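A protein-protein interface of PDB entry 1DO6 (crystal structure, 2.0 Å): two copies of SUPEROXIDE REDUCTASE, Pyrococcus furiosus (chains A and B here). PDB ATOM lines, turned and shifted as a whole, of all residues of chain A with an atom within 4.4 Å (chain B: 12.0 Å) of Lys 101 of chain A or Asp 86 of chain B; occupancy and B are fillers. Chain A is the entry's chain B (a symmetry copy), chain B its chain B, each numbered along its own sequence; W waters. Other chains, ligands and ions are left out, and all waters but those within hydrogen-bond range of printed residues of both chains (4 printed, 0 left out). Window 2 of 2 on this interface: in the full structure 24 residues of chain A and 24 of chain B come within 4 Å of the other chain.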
ATOM      1  N   ARG A  24     -13.766  10.887  25.453  1.00  0.00           N
ATOM      2  CA  ARG A  24     -14.434  10.407  24.236  1.00  0.00           C
ATOM      3  C   ARG A  24     -15.819  11.053  24.160  1.00  0.00           C
ATOM      4  O   ARG A  24     -16.625  10.904  25.076  1.00  0.00           O
ATOM      5  CB  ARG A  24     -14.564   8.878  24.280  1.00  0.00           C
ATOM      6  CG  ARG A  24     -15.187   8.241  23.038  1.00  0.00           C
ATOM      7  CD  ARG A  24     -14.563   6.871  22.748  1.00  0.00           C
ATOM      8  NE  ARG A  24     -14.243   6.726  21.330  1.00  0.00           N
ATOM      9  CZ  ARG A  24     -13.384   5.842  20.837  1.00  0.00           C
ATOM     10  NH1 ARG A  24     -12.736   4.996  21.636  1.00  0.00           N
ATOM     11  NH2 ARG A  24     -13.162   5.818  19.535  1.00  0.00           N
ATOM     12  N   PHE A  56      -1.285   6.081  17.502  1.00  0.00           N
ATOM     13  CA  PHE A  56      -2.431   5.257  17.845  1.00  0.00           C
ATOM     14  C   PHE A  56      -2.319   3.921  17.141  1.00  0.00           C
ATOM     15  O   PHE A  56      -2.163   3.870  15.919  1.00  0.00           O
ATOM     16  CB  PHE A  56      -3.727   5.948  17.418  1.00  0.00           C
ATOM     17  CG  PHE A  56      -4.977   5.101  17.626  1.00  0.00           C
ATOM     18  CD1 PHE A  56      -5.169   4.381  18.810  1.00  0.00           C
ATOM     19  CD2 PHE A  56      -5.996   5.096  16.669  1.00  0.00           C
ATOM     20  CE1 PHE A  56      -6.350   3.680  19.049  1.00  0.00           C
ATOM     21  CE2 PHE A  56      -7.197   4.388  16.898  1.00  0.00           C
ATOM     22  CZ  PHE A  56      -7.369   3.685  18.091  1.00  0.00           C
ATOM     23  N   PRO A  58      -4.567   0.843  16.561  1.00  0.00           N
ATOM     24  CA  PRO A  58      -5.905   0.297  16.828  1.00  0.00           C
ATOM     25  C   PRO A  58      -5.868  -1.185  17.243  1.00  0.00           C
ATOM     26  O   PRO A  58      -4.988  -1.964  16.841  1.00  0.00           O
ATOM     27  CB  PRO A  58      -6.676   0.533  15.520  1.00  0.00           C
ATOM     28  CG  PRO A  58      -5.782   1.481  14.692  1.00  0.00           C
ATOM     29  CD  PRO A  58      -4.377   1.203  15.145  1.00  0.00           C
ATOM     30  N   GLU A  61      -4.734  -4.429  15.084  1.00  0.00           N
ATOM     31  CA  GLU A  61      -4.104  -4.094  13.809  1.00  0.00           C
ATOM     32  C   GLU A  61      -2.596  -4.182  13.905  1.00  0.00           C
ATOM     33  O   GLU A  61      -2.060  -4.294  14.998  1.00  0.00           O
ATOM     34  CB  GLU A  61      -4.580  -2.719  13.349  1.00  0.00           C
ATOM     35  CG  GLU A  61      -6.105  -2.682  13.208  1.00  0.00           C
ATOM     36  CD  GLU A  61      -6.624  -1.422  12.529  1.00  0.00           C
ATOM     37  OE1 GLU A  61      -5.797  -0.665  11.971  1.00  0.00           O
ATOM     38  OE2 GLU A  61      -7.863  -1.192  12.555  1.00  0.00           O
ATOM     39  N   LYS A  98     -10.712  11.730  15.327  1.00  0.00           N
ATOM     40  CA  LYS A  98     -12.024  11.226  14.937  1.00  0.00           C
ATOM     41  C   LYS A  98     -11.877   9.738  14.641  1.00  0.00           C
ATOM     42  O   LYS A  98     -11.240   9.345  13.660  1.00  0.00           O
ATOM     43  CB  LYS A  98     -12.525  11.943  13.686  1.00  0.00           C
ATOM     44  CG  LYS A  98     -13.995  11.709  13.408  1.00  0.00           C
ATOM     45  CD  LYS A  98     -14.596  12.906  12.679  1.00  0.00           C
ATOM     46  CE  LYS A  98     -14.961  12.557  11.249  1.00  0.00           C
ATOM     47  NZ  LYS A  98     -13.837  12.832  10.300  1.00  0.00           N
ATOM     48  N   THR A  99     -12.442   8.911  15.506  1.00  0.00           N
ATOM     49  CA  THR A  99     -12.364   7.473  15.311  1.00  0.00           C
ATOM     50  C   THR A  99     -13.361   6.747  16.200  1.00  0.00           C
ATOM     51  O   THR A  99     -13.752   7.249  17.258  1.00  0.00           O
ATOM     52  CB  THR A  99     -10.953   6.929  15.626  1.00  0.00           C
ATOM     53  OG1 THR A  99     -10.858   5.566  15.183  1.00  0.00           O
ATOM     54  CG2 THR A  99     -10.679   6.990  17.146  1.00  0.00           C
ATOM     55  N   LYS A 100     -13.784   5.569  15.768  1.00  0.00           N
ATOM     56  CA  LYS A 100     -14.707   4.794  16.585  1.00  0.00           C
ATOM     57  C   LYS A 100     -13.947   3.583  17.114  1.00  0.00           C
ATOM     58  O   LYS A 100     -14.453   2.827  17.929  1.00  0.00           O
ATOM     59  CB  LYS A 100     -15.927   4.362  15.760  1.00  0.00           C
ATOM     60  CG  LYS A 100     -16.854   5.530  15.429  1.00  0.00           C
ATOM     61  CD  LYS A 100     -18.152   5.069  14.770  1.00  0.00           C
ATOM     62  CE  LYS A 100     -18.224   5.465  13.286  1.00  0.00           C
ATOM     63  NZ  LYS A 100     -16.904   5.426  12.570  1.00  0.00           N
ATOM     64  N   LYS A 101     -12.702   3.432  16.664  1.00  0.00           N
ATOM     65  CA  LYS A 101     -11.874   2.320  17.092  1.00  0.00           C
ATOM     66  C   LYS A 101     -11.343   2.467  18.511  1.00  0.00           C
ATOM     67  O   LYS A 101     -11.397   3.539  19.122  1.00  0.00           O
ATOM     68  CB  LYS A 101     -10.712   2.141  16.122  1.00  0.00           C
ATOM     69  CG  LYS A 101     -11.174   1.889  14.694  1.00  0.00           C
ATOM     70  CD  LYS A 101     -10.031   1.473  13.800  1.00  0.00           C
ATOM     71  CE  LYS A 101     -10.549   0.939  12.467  1.00  0.00           C
ATOM     72  NZ  LYS A 101      -9.414   0.666  11.532  1.00  0.00           N
ATOM     73  N   LYS A 102     -10.844   1.365  19.038  1.00  0.00           N
ATOM     74  CA  LYS A 102     -10.263   1.339  20.363  1.00  0.00           C
ATOM     75  C   LYS A 102      -8.855   0.846  20.116  1.00  0.00           C
ATOM     76  O   LYS A 102      -8.552   0.324  19.037  1.00  0.00           O
ATOM     77  CB  LYS A 102     -11.026   0.364  21.268  1.00  0.00           C
ATOM     78  CG  LYS A 102     -12.529   0.580  21.238  1.00  0.00           C
ATOM     79  CD  LYS A 102     -13.205   0.017  22.471  1.00  0.00           C
ATOM     80  CE  LYS A 102     -13.448  -1.485  22.335  1.00  0.00           C
ATOM     81  NZ  LYS A 102     -14.912  -1.825  22.424  1.00  0.00           N
ATOM     82  N   LEU A 123      -6.947   3.219  24.914  1.00  0.00           N
ATOM     83  CA  LEU A 123      -8.099   3.976  24.472  1.00  0.00           C
ATOM     84  C   LEU A 123      -9.312   3.043  24.478  1.00  0.00           C
ATOM     85  O   LEU A 123      -9.340   2.062  23.729  1.00  0.00           O
ATOM     86  CB  LEU A 123      -7.862   4.508  23.061  1.00  0.00           C
ATOM     87  CG  LEU A 123      -9.064   5.191  22.415  1.00  0.00           C
ATOM     88  CD1 LEU A 123      -9.676   6.195  23.372  1.00  0.00           C
ATOM     89  CD2 LEU A 123      -8.618   5.871  21.138  1.00  0.00           C
ATOM     90  N   ASN B  43     -11.710  16.258   5.240  1.00  0.00           N
ATOM     91  CA  ASN B  43     -10.574  15.577   5.846  1.00  0.00           C
ATOM     92  C   ASN B  43     -10.571  14.159   5.241  1.00  0.00           C
ATOM     93  O   ASN B  43     -11.116  13.234   5.827  1.00  0.00           O
ATOM     94  CB  ASN B  43     -10.715  15.511   7.379  1.00  0.00           C
ATOM     95  CG  ASN B  43      -9.428  15.085   8.055  1.00  0.00           C
ATOM     96  OD1 ASN B  43      -8.462  14.707   7.386  1.00  0.00           O
ATOM     97  ND2 ASN B  43      -9.400  15.154   9.388  1.00  0.00           N
ATOM     98  N   THR B  44      -9.964  14.018   4.064  1.00  0.00           N
ATOM     99  CA  THR B  44      -9.897  12.738   3.361  1.00  0.00           C
ATOM    100  C   THR B  44      -8.467  12.503   2.980  1.00  0.00           C
ATOM    101  O   THR B  44      -7.635  13.407   3.080  1.00  0.00           O
ATOM    102  CB  THR B  44     -10.731  12.759   2.042  1.00  0.00           C
ATOM    103  OG1 THR B  44     -10.238  13.791   1.182  1.00  0.00           O
ATOM    104  CG2 THR B  44     -12.166  13.027   2.336  1.00  0.00           C
ATOM    105  N   THR B  45      -8.184  11.294   2.519  1.00  0.00           N
ATOM    106  CA  THR B  45      -6.849  10.939   2.121  1.00  0.00           C
ATOM    107  C   THR B  45      -6.337  11.840   1.000  1.00  0.00           C
ATOM    108  O   THR B  45      -5.144  12.192   0.958  1.00  0.00           O
ATOM    109  CB  THR B  45      -6.783   9.439   1.697  1.00  0.00           C
ATOM    110  OG1 THR B  45      -7.166   8.601   2.804  1.00  0.00           O
ATOM    111  CG2 THR B  45      -5.368   9.069   1.243  1.00  0.00           C
ATOM    112  N   GLU B  46      -7.218  12.258   0.099  1.00  0.00           N
ATOM    113  CA  GLU B  46      -6.749  13.082  -1.003  1.00  0.00           C
ATOM    114  C   GLU B  46      -6.842  14.597  -0.801  1.00  0.00           C
ATOM    115  O   GLU B  46      -6.226  15.360  -1.550  1.00  0.00           O
ATOM    116  CB  GLU B  46      -7.475  12.694  -2.310  1.00  0.00           C
ATOM    117  CG  GLU B  46      -8.952  12.423  -2.173  1.00  0.00           C
ATOM    118  CD  GLU B  46      -9.255  11.016  -1.651  1.00  0.00           C
ATOM    119  OE1 GLU B  46      -8.904  10.022  -2.332  1.00  0.00           O
ATOM    120  OE2 GLU B  46      -9.841  10.920  -0.552  1.00  0.00           O
ATOM    121  N   THR B  73      -1.701  14.502  11.123  1.00  0.00           N
ATOM    122  CA  THR B  73      -1.128  13.475  10.268  1.00  0.00           C
ATOM    123  C   THR B  73      -1.944  12.251   9.871  1.00  0.00           C
ATOM    124  O   THR B  73      -1.465  11.438   9.091  1.00  0.00           O
ATOM    125  CB  THR B  73       0.190  12.985  10.898  1.00  0.00           C
ATOM    126  OG1 THR B  73      -0.078  12.548  12.231  1.00  0.00           O
ATOM    127  CG2 THR B  73       1.215  14.146  10.991  1.00  0.00           C
ATOM    128  N   ALA B  74      -3.138  12.082  10.419  1.00  0.00           N
ATOM    129  CA  ALA B  74      -3.937  10.914  10.029  1.00  0.00           C
ATOM    130  C   ALA B  74      -5.121  11.408   9.215  1.00  0.00           C
ATOM    131  O   ALA B  74      -5.875  12.296   9.655  1.00  0.00           O
ATOM    132  CB  ALA B  74      -4.423  10.166  11.241  1.00  0.00           C
ATOM    133  N   HIS B  75      -5.280  10.842   8.023  1.00  0.00           N
ATOM    134  CA  HIS B  75      -6.398  11.217   7.141  1.00  0.00           C
ATOM    135  C   HIS B  75      -7.114  10.014   6.456  1.00  0.00           C
ATOM    136  O   HIS B  75      -7.452  10.087   5.270  1.00  0.00           O
ATOM    137  CB  HIS B  75      -5.890  12.195   6.076  1.00  0.00           C
ATOM    138  CG  HIS B  75      -5.156  13.361   6.663  1.00  0.00           C
ATOM    139  ND1 HIS B  75      -3.780  13.444   6.686  1.00  0.00           N
ATOM    140  CD2 HIS B  75      -5.612  14.440   7.340  1.00  0.00           C
ATOM    141  CE1 HIS B  75      -3.419  14.527   7.355  1.00  0.00           C
ATOM    142  NE2 HIS B  75      -4.510  15.148   7.761  1.00  0.00           N
ATOM    143  N   GLY B  76      -7.320   8.937   7.215  1.00  0.00           N
ATOM    144  CA  GLY B  76      -8.027   7.766   6.717  1.00  0.00           C
ATOM    145  C   GLY B  76      -7.290   6.718   5.924  1.00  0.00           C
ATOM    146  O   GLY B  76      -7.857   5.672   5.633  1.00  0.00           O
ATOM    147  N   GLU B  77      -6.038   6.971   5.565  1.00  0.00           N
ATOM    148  CA  GLU B  77      -5.274   6.010   4.779  1.00  0.00           C
ATOM    149  C   GLU B  77      -5.003   4.695   5.532  1.00  0.00           C
ATOM    150  O   GLU B  77      -4.800   4.686   6.755  1.00  0.00           O
ATOM    151  CB  GLU B  77      -3.946   6.646   4.331  1.00  0.00           C
ATOM    152  CG  GLU B  77      -3.022   7.110   5.504  1.00  0.00           C
ATOM    153  CD  GLU B  77      -3.422   8.475   6.117  1.00  0.00           C
ATOM    154  OE1 GLU B  77      -3.982   9.326   5.399  1.00  0.00           O
ATOM    155  OE2 GLU B  77      -3.169   8.699   7.328  1.00  0.00           O
ATOM    156  N   SER B  78      -5.017   3.576   4.809  1.00  0.00           N
ATOM    157  CA  SER B  78      -4.709   2.280   5.423  1.00  0.00           C
ATOM    158  C   SER B  78      -4.334   1.322   4.311  1.00  0.00           C
ATOM    159  O   SER B  78      -4.444   1.671   3.135  1.00  0.00           O
ATOM    160  CB  SER B  78      -5.901   1.734   6.235  1.00  0.00           C
ATOM    161  OG  SER B  78      -6.744   0.881   5.461  1.00  0.00           O
ATOM    162  N   VAL B  79      -3.842   0.141   4.674  1.00  0.00           N
ATOM    163  CA  VAL B  79      -3.476  -0.857   3.681  1.00  0.00           C
ATOM    164  C   VAL B  79      -4.745  -1.275   2.897  1.00  0.00           C
ATOM    165  O   VAL B  79      -4.659  -1.914   1.855  1.00  0.00           O
ATOM    166  CB  VAL B  79      -2.889  -2.121   4.355  1.00  0.00           C
ATOM    167  CG1 VAL B  79      -1.472  -1.838   4.874  1.00  0.00           C
ATOM    168  CG2 VAL B  79      -3.810  -2.554   5.502  1.00  0.00           C
ATOM    169  N   ASN B  80      -5.922  -0.914   3.398  1.00  0.00           N
ATOM    170  CA  ASN B  80      -7.148  -1.283   2.699  1.00  0.00           C
ATOM    171  C   ASN B  80      -7.622  -0.224   1.708  1.00  0.00           C
ATOM    172  O   ASN B  80      -8.679  -0.352   1.087  1.00  0.00           O
ATOM    173  CB  ASN B  80      -8.240  -1.612   3.708  1.00  0.00           C
ATOM    174  CG  ASN B  80      -8.047  -2.989   4.308  1.00  0.00           C
ATOM    175  OD1 ASN B  80      -7.532  -3.903   3.642  1.00  0.00           O
ATOM    176  ND2 ASN B  80      -8.436  -3.145   5.555  1.00  0.00           N
ATOM    177  N   GLY B  81      -6.815   0.820   1.552  1.00  0.00           N
ATOM    178  CA  GLY B  81      -7.154   1.867   0.622  1.00  0.00           C
ATOM    179  C   GLY B  81      -7.390   3.217   1.275  1.00  0.00           C
ATOM    180  O   GLY B  81      -7.440   3.346   2.502  1.00  0.00           O
ATOM    181  N   PRO B  82      -7.550   4.261   0.451  1.00  0.00           N
ATOM    182  CA  PRO B  82      -7.785   5.604   0.972  1.00  0.00           C
ATOM    183  C   PRO B  82      -9.094   5.656   1.727  1.00  0.00           C
ATOM    184  O   PRO B  82     -10.034   4.940   1.401  1.00  0.00           O
ATOM    185  CB  PRO B  82      -7.806   6.481  -0.277  1.00  0.00           C
ATOM    186  CG  PRO B  82      -8.096   5.519  -1.427  1.00  0.00           C
ATOM    187  CD  PRO B  82      -7.503   4.223  -1.026  1.00  0.00           C
ATOM    188  N   ASN B  83      -9.140   6.485   2.762  1.00  0.00           N
ATOM    189  CA  ASN B  83     -10.343   6.666   3.559  1.00  0.00           C
ATOM    190  C   ASN B  83     -10.936   5.389   4.153  1.00  0.00           C
ATOM    191  O   ASN B  83     -12.154   5.285   4.262  1.00  0.00           O
ATOM    192  CB  ASN B  83     -11.423   7.376   2.719  1.00  0.00           C
ATOM    193  CG  ASN B  83     -10.906   8.632   2.042  1.00  0.00           C
ATOM    194  OD1 ASN B  83     -10.849   8.729   0.804  1.00  0.00           O
ATOM    195  ND2 ASN B  83     -10.517   9.601   2.847  1.00  0.00           N
ATOM    196  N   THR B  84     -10.097   4.442   4.558  1.00  0.00           N
ATOM    197  CA  THR B  84     -10.589   3.191   5.147  1.00  0.00           C
ATOM    198  C   THR B  84     -10.150   2.956   6.600  1.00  0.00           C
ATOM    199  O   THR B  84     -10.688   2.072   7.267  1.00  0.00           O
ATOM    200  CB  THR B  84     -10.113   1.988   4.330  1.00  0.00           C
ATOM    201  OG1 THR B  84      -8.678   2.015   4.260  1.00  0.00           O
ATOM    202  CG2 THR B  84     -10.665   2.068   2.883  1.00  0.00           C
ATOM    203  N   SER B  85      -9.192   3.742   7.101  1.00  0.00           N
ATOM    204  CA  SER B  85      -8.682   3.530   8.469  1.00  0.00           C
ATOM    205  C   SER B  85      -9.601   3.894   9.617  1.00  0.00           C
ATOM    206  O   SER B  85      -9.474   3.347  10.718  1.00  0.00           O
ATOM    207  CB  SER B  85      -7.372   4.307   8.673  1.00  0.00           C
ATOM    208  OG  SER B  85      -7.667   5.673   8.962  1.00  0.00           O
ATOM    209  N   ASP B  86     -10.521   4.816   9.380  1.00  0.00           N
ATOM    210  CA  ASP B  86     -11.412   5.334  10.419  1.00  0.00           C
ATOM    211  C   ASP B  86     -10.616   6.110  11.494  1.00  0.00           C
ATOM    212  O   ASP B  86     -11.035   6.204  12.660  1.00  0.00           O
ATOM    213  CB  ASP B  86     -12.224   4.244  11.112  1.00  0.00           C
ATOM    214  CG  ASP B  86     -13.345   4.833  11.949  1.00  0.00           C
ATOM    215  OD1 ASP B  86     -13.549   4.399  13.104  1.00  0.00           O
ATOM    216  OD2 ASP B  86     -14.019   5.768  11.456  1.00  0.00           O
ATOM    217  N   VAL B  87      -9.461   6.645  11.095  1.00  0.00           N
ATOM    218  CA  VAL B  87      -8.626   7.443  12.001  1.00  0.00           C
ATOM    219  C   VAL B  87      -8.336   8.765  11.274  1.00  0.00           C
ATOM    220  O   VAL B  87      -7.643   8.786  10.248  1.00  0.00           O
ATOM    221  CB  VAL B  87      -7.293   6.747  12.311  1.00  0.00           C
ATOM    222  CG1 VAL B  87      -6.448   7.631  13.250  1.00  0.00           C
ATOM    223  CG2 VAL B  87      -7.547   5.399  12.953  1.00  0.00           C
ATOM    224  N   TYR B  88      -8.880   9.855  11.810  1.00  0.00           N
ATOM    225  CA  TYR B  88      -8.701  11.175  11.215  1.00  0.00           C
ATOM    226  C   TYR B  88      -8.311  12.221  12.249  1.00  0.00           C
ATOM    227  O   TYR B  88      -8.908  12.287  13.326  1.00  0.00           O
ATOM    228  CB  TYR B  88     -10.003  11.638  10.540  1.00  0.00           C
ATOM    229  CG  TYR B  88     -10.433  10.747   9.403  1.00  0.00           C
ATOM    230  CD1 TYR B  88     -11.218   9.612   9.639  1.00  0.00           C
ATOM    231  CD2 TYR B  88     -10.035  11.018   8.091  1.00  0.00           C
ATOM    232  CE1 TYR B  88     -11.599   8.766   8.589  1.00  0.00           C
ATOM    233  CE2 TYR B  88     -10.410  10.179   7.033  1.00  0.00           C
ATOM    234  CZ  TYR B  88     -11.189   9.060   7.292  1.00  0.00           C
ATOM    235  OH  TYR B  88     -11.565   8.249   6.251  1.00  0.00           O
ATOM    236  N   THR B  89      -7.310  13.032  11.933  1.00  0.00           N
ATOM    237  CA  THR B  89      -6.936  14.097  12.873  1.00  0.00           C
ATOM    238  C   THR B  89      -7.583  15.395  12.419  1.00  0.00           C
ATOM    239  O   THR B  89      -7.290  15.879  11.325  1.00  0.00           O
ATOM    240  CB  THR B  89      -5.441  14.325  12.906  1.00  0.00           C
ATOM    241  OG1 THR B  89      -4.779  13.076  13.118  1.00  0.00           O
ATOM    242  CG2 THR B  89      -5.096  15.323  14.042  1.00  0.00           C
ATOM    243  N   GLU B  90      -8.453  15.955  13.257  1.00  0.00           N
ATOM    244  CA  GLU B  90      -9.151  17.192  12.919  1.00  0.00           C
ATOM    245  C   GLU B  90      -8.214  18.410  13.028  1.00  0.00           C
ATOM    246  O   GLU B  90      -7.348  18.450  13.911  1.00  0.00           O
ATOM    247  CB  GLU B  90     -10.370  17.334  13.825  1.00  0.00           C
ATOM    248  CG  GLU B  90     -11.504  16.357  13.443  1.00  0.00           C
ATOM    249  CD  GLU B  90     -11.986  16.573  11.998  1.00  0.00           C
ATOM    250  OE1 GLU B  90     -12.758  17.525  11.766  1.00  0.00           O
ATOM    251  OE2 GLU B  90     -11.585  15.810  11.088  1.00  0.00           O
HETATM  252  O   HOH W   1     -13.877  15.049   9.345  1.00  0.00           O
HETATM  253  O   HOH W   2     -10.675   0.194   9.229  1.00  0.00           O
HETATM  254  O   HOH W   3     -13.604   8.370  12.074  1.00  0.00           O
HETATM  255  O   HOH W   4     -13.390  12.316   7.581  1.00  0.00           O
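The backbone NH of Ser 85 of chain B is in hydrogen-bond range of the backbone carbonyl oxygen of Gly 76 of chain B (2.8 Å). The backbone NH of Gly 76 of chain B lies within hydrogen-bond range of the backbone carbonyl oxygen of Val 87 of chain B (3.1 Å). The side-chain hydroxyl of Ser 85 of chain B is in hydrogen-bond range of the backbone NH of Val 87 of chain B, 3.0 Å away. The backbone carbonyl oxygen of Thr 99 of chain A lies within hydrogen-bond range of the guanidinium group of Arg 24 of chain A, at 2.8 Å. OE2 of Glu 61 of chain A is in salt-bridge range of NZ of Lys 101 of chain A. The side-chain hydroxyl of Thr 99 of chain A lies within hydrogen-bond range of the backbone NH of Lys 101 of chain A (3.2 Å).
Of the printed residues of chain B, Thr 99 of chain A touches Asp 86 and Val 87. Of chain B, only Asp 86 comes within 4 Å of Lys 100 of chain A. Of the printed residues of chain B, Lys 101 of chain A touches Ser 85 and Asp 86. Lys 102 of chain A touches none of the printed residues of chain B. No residue of chain B comes within 4 Å of Leu 123 of chain A. Of chain A, only Lys 98 (3.3 Å), Thr 99 (2.6 Å), Lys 100 (2.9 Å) and Lys 101 (3.8 Å) come within 4 Å of Asp 86 of chain B. Printed residues of chain A within 4 Å of Val 87 of chain B: Lys 98 (3.6 Å) and Thr 99 (3.995 Å). Of the printed residues of chain A, Tyr 88 of chain B touches Lys 98. Printed residues of chain A within 4 Å of Glu 90 of chain B: Lys 98.
No position is printed for both chains.
The side-chain amino group (NZ) of Lys 101 of chain A lies within hydrogen-bond range of the backbone carbonyl oxygen (O) of Ser 85 of chain B (2.8 Å). OG1 of Thr 99 of chain A lies within hydrogen-bond range of O of Asp 86 of chain B, 2.6 Å away. The side-chain amino group of Lys 100 of chain A is in salt-bridge range of the side-chain carboxylate of Asp 86 of chain B, 3.1 Å away. O of Tyr 88 of chain B lies within hydrogen-bond range of N of Lys 98 of chain A (2.8 Å). The side-chain carboxylate (OE2) of Glu 90 of chain B lies within salt-bridge range of the side-chain amino group (NZ) of Lys 98 of chain A, 3.8 Å away. O of Asp 86 of chain B lies close to O of Lys 98 of chain A (3.3 Å).
Among the printed residues, merely in contact across the chains: Lys 98 of chain A with Val 87 of chain B (3.6 Å), Lys 101 of chain A with Asp 86 of chain B (3.8 Å) and Thr 99 of chain A with Val 87 of chain B (3.995 Å).
Water W1 lies within hydrogen-bond range of NZ of Lys 98 of chain A (2.4 Å) and OE2 of Glu 90 of chain B (3.0 Å). Water W2 bridges the side-chain amino group (NZ) of Lys 101 of chain A (2.7 Å) and the backbone carbonyl oxygen (O) of Thr 84 of chain B (2.7 Å). Water W3 bridges the side-chain carboxylate of Asp 86 of chain B (2.7 Å) and the backbone carbonyl oxygen of Lys 98 of chain A (3.0 Å). Water W4 bridges NZ of Lys 98 of chain A and O of Asn 43 of chain B.
Among the printed residues, Asp or Glu carboxylates within 4 Å of a Lys or Arg side-chain nitrogen of the other chain: Lys 98 of chain A with Glu 90 of chain B (3.8 Å) and Lys 100 of chain A with Asp 86 of chain B (3.1 Å).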
